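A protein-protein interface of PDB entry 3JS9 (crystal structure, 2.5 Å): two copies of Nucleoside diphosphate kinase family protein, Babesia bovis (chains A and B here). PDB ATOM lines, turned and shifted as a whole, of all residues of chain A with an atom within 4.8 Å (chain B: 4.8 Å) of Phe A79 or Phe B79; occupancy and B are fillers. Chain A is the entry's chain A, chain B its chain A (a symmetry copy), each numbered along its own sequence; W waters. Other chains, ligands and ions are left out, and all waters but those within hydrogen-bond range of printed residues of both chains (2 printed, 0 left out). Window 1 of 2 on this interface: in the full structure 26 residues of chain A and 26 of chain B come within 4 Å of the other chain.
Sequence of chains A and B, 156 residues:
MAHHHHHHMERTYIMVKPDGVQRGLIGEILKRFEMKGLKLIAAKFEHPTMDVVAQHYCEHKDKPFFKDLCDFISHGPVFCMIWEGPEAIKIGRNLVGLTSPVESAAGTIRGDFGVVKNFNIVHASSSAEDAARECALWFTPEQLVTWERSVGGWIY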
ATOM      1  N   ILE A  14       5.877  25.867  -9.282  1.00  0.00           N
ATOM      2  CA  ILE A  14       5.145  25.860  -8.013  1.00  0.00           C
ATOM      3  C   ILE A  14       5.618  24.617  -7.216  1.00  0.00           C
ATOM      4  O   ILE A  14       5.657  23.506  -7.758  1.00  0.00           O
ATOM      5  CB  ILE A  14       3.560  25.825  -8.239  1.00  0.00           C
ATOM      6  CG1 ILE A  14       3.047  26.938  -9.183  1.00  0.00           C
ATOM      7  CG2 ILE A  14       2.758  25.734  -6.900  1.00  0.00           C
ATOM      8  CD1 ILE A  14       3.066  28.426  -8.673  1.00  0.00           C
ATOM      9  N   MET A  15       5.929  24.796  -5.930  1.00  0.00           N
ATOM     10  CA  MET A  15       6.477  23.698  -5.160  1.00  0.00           C
ATOM     11  C   MET A  15       5.861  23.557  -3.760  1.00  0.00           C
ATOM     12  O   MET A  15       5.951  24.460  -2.905  1.00  0.00           O
ATOM     13  CB  MET A  15       8.004  23.815  -5.079  1.00  0.00           C
ATOM     14  CG  MET A  15       8.659  22.665  -4.306  1.00  0.00           C
ATOM     15  SD  MET A  15      10.483  22.686  -4.212  1.00  0.00           S
ATOM     16  CE  MET A  15      10.756  24.361  -3.559  1.00  0.00           C
ATOM     17  N   VAL A  16       5.218  22.430  -3.519  1.00  0.00           N
ATOM     18  CA  VAL A  16       4.751  22.148  -2.177  1.00  0.00           C
ATOM     19  C   VAL A  16       5.996  21.783  -1.375  1.00  0.00           C
ATOM     20  O   VAL A  16       6.717  20.840  -1.743  1.00  0.00           O
ATOM     21  CB  VAL A  16       3.758  20.977  -2.136  1.00  0.00           C
ATOM     22  CG1 VAL A  16       3.235  20.777  -0.705  1.00  0.00           C
ATOM     23  CG2 VAL A  16       2.644  21.242  -3.101  1.00  0.00           C
ATOM     24  N   VAL A  21       3.741  19.027   2.657  1.00  0.00           N
ATOM     25  CA  VAL A  21       3.599  17.604   2.450  1.00  0.00           C
ATOM     26  C   VAL A  21       3.222  16.897   3.735  1.00  0.00           C
ATOM     27  O   VAL A  21       2.322  16.047   3.730  1.00  0.00           O
ATOM     28  CB  VAL A  21       4.865  16.967   1.843  1.00  0.00           C
ATOM     29  CG1 VAL A  21       4.767  15.429   1.851  1.00  0.00           C
ATOM     30  CG2 VAL A  21       5.131  17.523   0.409  1.00  0.00           C
ATOM     31  N   ILE A  26      -0.845  18.448  -0.474  1.00  0.00           N
ATOM     32  CA  ILE A  26      -0.423  18.371  -1.871  1.00  0.00           C
ATOM     33  C   ILE A  26      -1.638  18.453  -2.770  1.00  0.00           C
ATOM     34  O   ILE A  26      -1.661  19.261  -3.732  1.00  0.00           O
ATOM     35  CB  ILE A  26       0.361  17.079  -2.231  1.00  0.00           C
ATOM     36  CG1 ILE A  26       1.682  17.013  -1.447  1.00  0.00           C
ATOM     37  CG2 ILE A  26       0.579  16.990  -3.768  1.00  0.00           C
ATOM     38  CD1 ILE A  26       2.343  15.616  -1.421  1.00  0.00           C
ATOM     39  N   LEU A  30      -2.584  21.349  -5.589  1.00  0.00           N
ATOM     40  CA  LEU A  30      -2.696  20.977  -6.996  1.00  0.00           C
ATOM     41  C   LEU A  30      -4.093  21.365  -7.522  1.00  0.00           C
ATOM     42  O   LEU A  30      -4.236  22.043  -8.536  1.00  0.00           O
ATOM     43  CB  LEU A  30      -2.415  19.479  -7.177  1.00  0.00           C
ATOM     44  CG  LEU A  30      -1.943  18.975  -8.567  1.00  0.00           C
ATOM     45  CD1 LEU A  30      -1.412  17.573  -8.452  1.00  0.00           C
ATOM     46  CD2 LEU A  30      -2.990  19.045  -9.721  1.00  0.00           C
ATOM     47  N   ALA A  43       4.930  17.536 -13.207  1.00  0.00           N
ATOM     48  CA  ALA A  43       4.737  17.361 -11.787  1.00  0.00           C
ATOM     49  C   ALA A  43       5.521  16.141 -11.385  1.00  0.00           C
ATOM     50  O   ALA A  43       5.624  15.210 -12.196  1.00  0.00           O
ATOM     51  CB  ALA A  43       3.254  17.151 -11.483  1.00  0.00           C
ATOM     52  N   LYS A  44       6.064  16.135 -10.164  1.00  0.00           N
ATOM     53  CA  LYS A  44       6.667  14.926  -9.557  1.00  0.00           C
ATOM     54  C   LYS A  44       6.890  15.091  -8.051  1.00  0.00           C
ATOM     55  O   LYS A  44       7.218  16.170  -7.581  1.00  0.00           O
ATOM     56  CB  LYS A  44       8.018  14.598 -10.208  1.00  0.00           C
ATOM     57  CG  LYS A  44       9.015  15.751 -10.147  1.00  0.00           C
ATOM     58  CD  LYS A  44      10.328  15.390 -10.754  1.00  0.00           C
ATOM     59  CE  LYS A  44      11.255  16.591 -10.832  1.00  0.00           C
ATOM     60  NZ  LYS A  44      12.384  16.327 -11.807  1.00  0.00           N
ATOM     61  N   PHE A  45       6.715  14.001  -7.306  1.00  0.00           N
ATOM     62  CA  PHE A  45       7.057  13.931  -5.893  1.00  0.00           C
ATOM     63  C   PHE A  45       8.565  13.598  -5.851  1.00  0.00           C
ATOM     64  O   PHE A  45       9.015  12.744  -6.593  1.00  0.00           O
ATOM     65  CB  PHE A  45       6.246  12.779  -5.269  1.00  0.00           C
ATOM     66  CG  PHE A  45       6.254  12.731  -3.759  1.00  0.00           C
ATOM     67  CD1 PHE A  45       6.090  13.898  -2.988  1.00  0.00           C
ATOM     68  CD2 PHE A  45       6.380  11.510  -3.110  1.00  0.00           C
ATOM     69  CE1 PHE A  45       6.062  13.851  -1.617  1.00  0.00           C
ATOM     70  CE2 PHE A  45       6.360  11.437  -1.701  1.00  0.00           C
ATOM     71  CZ  PHE A  45       6.193  12.611  -0.954  1.00  0.00           C
ATOM     72  N   PRO A  77      10.337  15.693   1.990  1.00  0.00           N
ATOM     73  CA  PRO A  77      10.109  15.615   0.556  1.00  0.00           C
ATOM     74  C   PRO A  77       9.424  16.892   0.037  1.00  0.00           C
ATOM     75  O   PRO A  77       8.941  17.701   0.847  1.00  0.00           O
ATOM     76  CB  PRO A  77       9.147  14.437   0.439  1.00  0.00           C
ATOM     77  CG  PRO A  77       8.436  14.427   1.719  1.00  0.00           C
ATOM     78  CD  PRO A  77       9.354  14.907   2.753  1.00  0.00           C
ATOM     79  N   VAL A  78       9.398  17.081  -1.279  1.00  0.00           N
ATOM     80  CA  VAL A  78       8.694  18.212  -1.873  1.00  0.00           C
ATOM     81  C   VAL A  78       7.844  17.738  -3.027  1.00  0.00           C
ATOM     82  O   VAL A  78       8.094  16.665  -3.562  1.00  0.00           O
ATOM     83  CB  VAL A  78       9.672  19.360  -2.341  1.00  0.00           C
ATOM     84  CG1 VAL A  78      10.538  19.825  -1.173  1.00  0.00           C
ATOM     85  CG2 VAL A  78      10.544  18.919  -3.544  1.00  0.00           C
ATOM     86  N   PHE A  79       6.844  18.526  -3.430  1.00  0.00           N
ATOM     87  CA  PHE A  79       6.087  18.185  -4.627  1.00  0.00           C
ATOM     88  C   PHE A  79       6.218  19.293  -5.642  1.00  0.00           C
ATOM     89  O   PHE A  79       5.840  20.431  -5.363  1.00  0.00           O
ATOM     90  CB  PHE A  79       4.635  17.864  -4.283  1.00  0.00           C
ATOM     91  CG  PHE A  79       3.809  17.407  -5.465  1.00  0.00           C
ATOM     92  CD1 PHE A  79       3.118  18.323  -6.236  1.00  0.00           C
ATOM     93  CD2 PHE A  79       3.696  16.054  -5.773  1.00  0.00           C
ATOM     94  CE1 PHE A  79       2.358  17.899  -7.315  1.00  0.00           C
ATOM     95  CE2 PHE A  79       2.930  15.625  -6.859  1.00  0.00           C
ATOM     96  CZ  PHE A  79       2.276  16.532  -7.629  1.00  0.00           C
ATOM     97  N   CYS A  80       6.761  18.955  -6.817  1.00  0.00           N
ATOM     98  CA  CYS A  80       7.150  19.915  -7.855  1.00  0.00           C
ATOM     99  C   CYS A  80       6.138  19.957  -8.960  1.00  0.00           C
ATOM    100  O   CYS A  80       5.670  18.902  -9.391  1.00  0.00           O
ATOM    101  CB  CYS A  80       8.480  19.510  -8.495  1.00  0.00           C
ATOM    102  SG  CYS A  80       9.830  19.086  -7.352  1.00  0.00           S
ATOM    103  N   MET A  81       5.845  21.164  -9.465  1.00  0.00           N
ATOM    104  CA  MET A  81       4.899  21.371 -10.574  1.00  0.00           C
ATOM    105  C   MET A  81       5.354  22.500 -11.460  1.00  0.00           C
ATOM    106  O   MET A  81       6.038  23.412 -10.987  1.00  0.00           O
ATOM    107  CB  MET A  81       3.492  21.731 -10.062  1.00  0.00           C
ATOM    108  CG  MET A  81       2.815  20.610  -9.269  1.00  0.00           C
ATOM    109  SD  MET A  81       1.453  21.303  -8.332  1.00  0.00           S
ATOM    110  CE  MET A  81       2.271  21.913  -6.816  1.00  0.00           C
ATOM    111  N   ILE B  14      -1.786   3.783  -8.571  1.00  0.00           N
ATOM    112  CA  ILE B  14      -3.024   4.505  -8.874  1.00  0.00           C
ATOM    113  C   ILE B  14      -2.720   5.466 -10.052  1.00  0.00           C
ATOM    114  O   ILE B  14      -1.727   6.203 -10.016  1.00  0.00           O
ATOM    115  CB  ILE B  14      -3.570   5.313  -7.603  1.00  0.00           C
ATOM    116  CG1 ILE B  14      -3.718   4.440  -6.335  1.00  0.00           C
ATOM    117  CG2 ILE B  14      -4.846   6.158  -7.924  1.00  0.00           C
ATOM    118  CD1 ILE B  14      -4.861   3.360  -6.294  1.00  0.00           C
ATOM    119  N   MET B  15      -3.591   5.490 -11.064  1.00  0.00           N
ATOM    120  CA  MET B  15      -3.310   6.288 -12.240  1.00  0.00           C
ATOM    121  C   MET B  15      -4.519   7.090 -12.746  1.00  0.00           C
ATOM    122  O   MET B  15      -5.566   6.534 -13.131  1.00  0.00           O
ATOM    123  CB  MET B  15      -2.731   5.406 -13.354  1.00  0.00           C
ATOM    124  CG  MET B  15      -2.375   6.190 -14.622  1.00  0.00           C
ATOM    125  SD  MET B  15      -1.619   5.233 -15.982  1.00  0.00           S
ATOM    126  CE  MET B  15      -2.847   3.904 -16.166  1.00  0.00           C
ATOM    127  N   VAL B  16      -4.389   8.403 -12.735  1.00  0.00           N
ATOM    128  CA  VAL B  16      -5.413   9.226 -13.346  1.00  0.00           C
ATOM    129  C   VAL B  16      -5.223   9.070 -14.852  1.00  0.00           C
ATOM    130  O   VAL B  16      -4.130   9.356 -15.373  1.00  0.00           O
ATOM    131  CB  VAL B  16      -5.277  10.708 -12.967  1.00  0.00           C
ATOM    132  CG1 VAL B  16      -6.433  11.518 -13.574  1.00  0.00           C
ATOM    133  CG2 VAL B  16      -5.237  10.833 -11.475  1.00  0.00           C
ATOM    134  N   VAL B  21      -7.679  13.535 -16.574  1.00  0.00           N
ATOM    135  CA  VAL B  21      -6.844  14.708 -16.707  1.00  0.00           C
ATOM    136  C   VAL B  21      -7.561  15.811 -17.456  1.00  0.00           C
ATOM    137  O   VAL B  21      -7.519  16.973 -17.029  1.00  0.00           O
ATOM    138  CB  VAL B  21      -5.493  14.396 -17.383  1.00  0.00           C
ATOM    139  CG1 VAL B  21      -4.730  15.692 -17.717  1.00  0.00           C
ATOM    140  CG2 VAL B  21      -4.641  13.434 -16.497  1.00  0.00           C
ATOM    141  N   ILE B  26      -7.235  15.618 -11.412  1.00  0.00           N
ATOM    142  CA  ILE B  26      -6.002  15.094 -10.826  1.00  0.00           C
ATOM    143  C   ILE B  26      -5.959  15.437  -9.353  1.00  0.00           C
ATOM    144  O   ILE B  26      -5.710  14.547  -8.502  1.00  0.00           O
ATOM    145  CB  ILE B  26      -4.703  15.630 -11.487  1.00  0.00           C
ATOM    146  CG1 ILE B  26      -4.623  15.189 -12.958  1.00  0.00           C
ATOM    147  CG2 ILE B  26      -3.457  15.188 -10.669  1.00  0.00           C
ATOM    148  CD1 ILE B  26      -3.601  15.974 -13.809  1.00  0.00           C
ATOM    149  N   LEU B  30      -5.909  12.866  -6.094  1.00  0.00           N
ATOM    150  CA  LEU B  30      -4.758  12.861  -5.197  1.00  0.00           C
ATOM    151  C   LEU B  30      -5.227  13.150  -3.756  1.00  0.00           C
ATOM    152  O   LEU B  30      -4.926  12.414  -2.820  1.00  0.00           O
ATOM    153  CB  LEU B  30      -3.708  13.876  -5.668  1.00  0.00           C
ATOM    154  CG  LEU B  30      -2.232  13.674  -5.233  1.00  0.00           C
ATOM    155  CD1 LEU B  30      -1.329  14.555  -6.051  1.00  0.00           C
ATOM    156  CD2 LEU B  30      -1.923  13.871  -3.718  1.00  0.00           C
ATOM    157  N   ALA B  43       4.992   9.999  -7.505  1.00  0.00           N
ATOM    158  CA  ALA B  43       3.980  10.611  -8.334  1.00  0.00           C
ATOM    159  C   ALA B  43       4.698  11.286  -9.472  1.00  0.00           C
ATOM    160  O   ALA B  43       5.816  11.774  -9.260  1.00  0.00           O
ATOM    161  CB  ALA B  43       3.196  11.644  -7.526  1.00  0.00           C
ATOM    162  N   LYS B  44       4.077  11.320 -10.655  1.00  0.00           N
ATOM    163  CA  LYS B  44       4.559  12.135 -11.794  1.00  0.00           C
ATOM    164  C   LYS B  44       3.497  12.275 -12.889  1.00  0.00           C
ATOM    165  O   LYS B  44       2.741  11.351 -13.149  1.00  0.00           O
ATOM    166  CB  LYS B  44       5.815  11.518 -12.422  1.00  0.00           C
ATOM    167  CG  LYS B  44       5.618  10.075 -12.875  1.00  0.00           C
ATOM    168  CD  LYS B  44       6.844   9.514 -13.512  1.00  0.00           C
ATOM    169  CE  LYS B  44       6.690   8.033 -13.813  1.00  0.00           C
ATOM    170  NZ  LYS B  44       8.043   7.397 -14.055  1.00  0.00           N
ATOM    171  N   PHE B  45       3.461  13.442 -13.530  1.00  0.00           N
ATOM    172  CA  PHE B  45       2.644  13.684 -14.711  1.00  0.00           C
ATOM    173  C   PHE B  45       3.481  13.166 -15.902  1.00  0.00           C
ATOM    174  O   PHE B  45       4.669  13.426 -15.963  1.00  0.00           O
ATOM    175  CB  PHE B  45       2.436  15.205 -14.835  1.00  0.00           C
ATOM    176  CG  PHE B  45       1.386  15.632 -15.834  1.00  0.00           C
ATOM    177  CD1 PHE B  45       0.143  14.975 -15.916  1.00  0.00           C
ATOM    178  CD2 PHE B  45       1.626  16.720 -16.663  1.00  0.00           C
ATOM    179  CE1 PHE B  45      -0.824  15.384 -16.798  1.00  0.00           C
ATOM    180  CE2 PHE B  45       0.649  17.155 -17.582  1.00  0.00           C
ATOM    181  CZ  PHE B  45      -0.583  16.488 -17.644  1.00  0.00           C
ATOM    182  N   PRO B  77      -2.420  12.569 -21.719  1.00  0.00           N
ATOM    183  CA  PRO B  77      -1.458  12.381 -20.644  1.00  0.00           C
ATOM    184  C   PRO B  77      -2.076  11.576 -19.487  1.00  0.00           C
ATOM    185  O   PRO B  77      -3.304  11.388 -19.458  1.00  0.00           O
ATOM    186  CB  PRO B  77      -1.192  13.811 -20.187  1.00  0.00           C
ATOM    187  CG  PRO B  77      -2.427  14.527 -20.512  1.00  0.00           C
ATOM    188  CD  PRO B  77      -3.000  13.922 -21.716  1.00  0.00           C
ATOM    189  N   VAL B  78      -1.247  11.096 -18.564  1.00  0.00           N
ATOM    190  CA  VAL B  78      -1.743  10.401 -17.382  1.00  0.00           C
ATOM    191  C   VAL B  78      -1.057  10.934 -16.148  1.00  0.00           C
ATOM    192  O   VAL B  78       0.007  11.531 -16.257  1.00  0.00           O
ATOM    193  CB  VAL B  78      -1.568   8.835 -17.479  1.00  0.00           C
ATOM    194  CG1 VAL B  78      -2.252   8.304 -18.736  1.00  0.00           C
ATOM    195  CG2 VAL B  78      -0.076   8.418 -17.436  1.00  0.00           C
ATOM    196  N   PHE B  79      -1.643  10.721 -14.967  1.00  0.00           N
ATOM    197  CA  PHE B  79      -0.954  11.087 -13.738  1.00  0.00           C
ATOM    198  C   PHE B  79      -0.755   9.859 -12.883  1.00  0.00           C
ATOM    199  O   PHE B  79      -1.729   9.212 -12.500  1.00  0.00           O
ATOM    200  CB  PHE B  79      -1.694  12.204 -13.006  1.00  0.00           C
ATOM    201  CG  PHE B  79      -0.987  12.703 -11.767  1.00  0.00           C
ATOM    202  CD1 PHE B  79      -1.236  12.129 -10.534  1.00  0.00           C
ATOM    203  CD2 PHE B  79      -0.103  13.777 -11.836  1.00  0.00           C
ATOM    204  CE1 PHE B  79      -0.589  12.593  -9.400  1.00  0.00           C
ATOM    205  CE2 PHE B  79       0.550  14.247 -10.694  1.00  0.00           C
ATOM    206  CZ  PHE B  79       0.321  13.660  -9.492  1.00  0.00           C
ATOM    207  N   CYS B  80       0.513   9.541 -12.597  1.00  0.00           N
ATOM    208  CA  CYS B  80       0.925   8.290 -11.951  1.00  0.00           C
ATOM    209  C   CYS B  80       1.229   8.505 -10.499  1.00  0.00           C
ATOM    210  O   CYS B  80       1.881   9.493 -10.158  1.00  0.00           O
ATOM    211  CB  CYS B  80       2.205   7.749 -12.591  1.00  0.00           C
ATOM    212  SG  CYS B  80       2.230   7.673 -14.408  1.00  0.00           S
ATOM    213  N   MET B  81       0.817   7.553  -9.649  1.00  0.00           N
ATOM    214  CA  MET B  81       1.068   7.599  -8.198  1.00  0.00           C
ATOM    215  C   MET B  81       1.312   6.216  -7.655  1.00  0.00           C
ATOM    216  O   MET B  81       0.804   5.240  -8.215  1.00  0.00           O
ATOM    217  CB  MET B  81      -0.133   8.185  -7.432  1.00  0.00           C
ATOM    218  CG  MET B  81      -0.416   9.654  -7.754  1.00  0.00           C
ATOM    219  SD  MET B  81      -2.077  10.057  -7.210  1.00  0.00           S
ATOM    220  CE  MET B  81      -3.108   9.525  -8.621  1.00  0.00           C
HETATM  221  O   HOH W   1       6.114  15.818 -15.307  1.00  0.00           O
HETATM  222  O   HOH W   2       7.942  10.217  -7.432  1.00  0.00           O
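Leu B30 touches its own counterpart, Leu A30. Ala A43 touches Lys B44, and with the chains exchanged Lys A44 touches Ala B43. Ala A43 touches Phe B45, and with the chains exchanged Phe A45 touches Ala B43. Phe A79 touches its own counterpart, Phe B79. Of the 8 pairs that touch across the chains among the printed residues, 8 have their exchanged pair printed and touching as well.
Ile A26 touches Leu B30. Leu A30 touches Ile B26. CD1 of Leu B30 touches CD1 of Leu A30, at 3.9 Å. O of Ala A43 touches CA of Lys B44, 3.3 Å away. O of Ala B43 touches CA of Lys A44 (3.3 Å). Phe B79 touches Phe A79.
The backbone NH of Val A16 is in hydrogen-bond range of the backbone carbonyl oxygen of Phe A79. N of Lys A44 is in hydrogen-bond range of O of Cys A80 (2.9 Å). The backbone NH of Val B16 is in hydrogen-bond range of the backbone carbonyl oxygen of Phe B79 (2.8 Å). The backbone NH (N) of Lys B44 sits at hydrogen-bond distance from the backbone carbonyl oxygen (O) of Cys B80, 2.9 Å away.
The backbone carbonyl oxygen (O) of Ala A43 lies within hydrogen-bond range of the backbone NH (N) of Phe B45. The backbone NH of Phe A45 is in hydrogen-bond range of the backbone carbonyl oxygen of Ala B43 (3.1 Å).
Of chain A, only Phe A79 (3.9 Å) comes within 4 Å of Phe B79. Of the printed residues of chain B, Phe A45 touches Ala B43. Of the printed residues of chain A, Ile B26 touches Leu A30. Of the printed residues of chain B, Lys A44 touches Ala B43. Printed residues of chain A within 4 Å of Leu B30: Ile A26 (3.8 Å) and Leu A30 (3.9 Å). Val B16 touches none of the printed residues of chain A. Val A16 touches none of the printed residues of chain B. The nearest residue of chain B that does not touch Phe A79 is Ala B43 (4.05 Å). The nearest residue of chain A that does not touch Phe B79 is Ala A43 (4.05 Å).
Water W1 lies within hydrogen-bond range of O of Phe B45 (2.9 Å) and N of Ala A43 (3.0 Å). Water W2 lies within hydrogen-bond range of the backbone carbonyl oxygen (O) of Phe A45 (2.9 Å) and the backbone NH (N) of Ala B43 (3.0 Å).
Of the 14 printed residues of chain A, 6 touch a printed residue of chain B. Printed residues of chain A that touch a printed residue of chain B: Ile A26, Leu A30, Ala A43, Lys A44, Phe A45 and Phe A79. Hydrophobic or aromatic side chains of chain A that line the printed part of chain B: Ile A26, Leu A30, Ala A43, Phe A45 and Phe A79. Of the 14 printed residues of chain B, 6 touch a printed residue of chain A. Hydrophobic or aromatic side chains of chain B within 4 Å of the printed part of chain A: Ile B26, Leu B30, Ala B43, Phe B45 and Phe B79.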
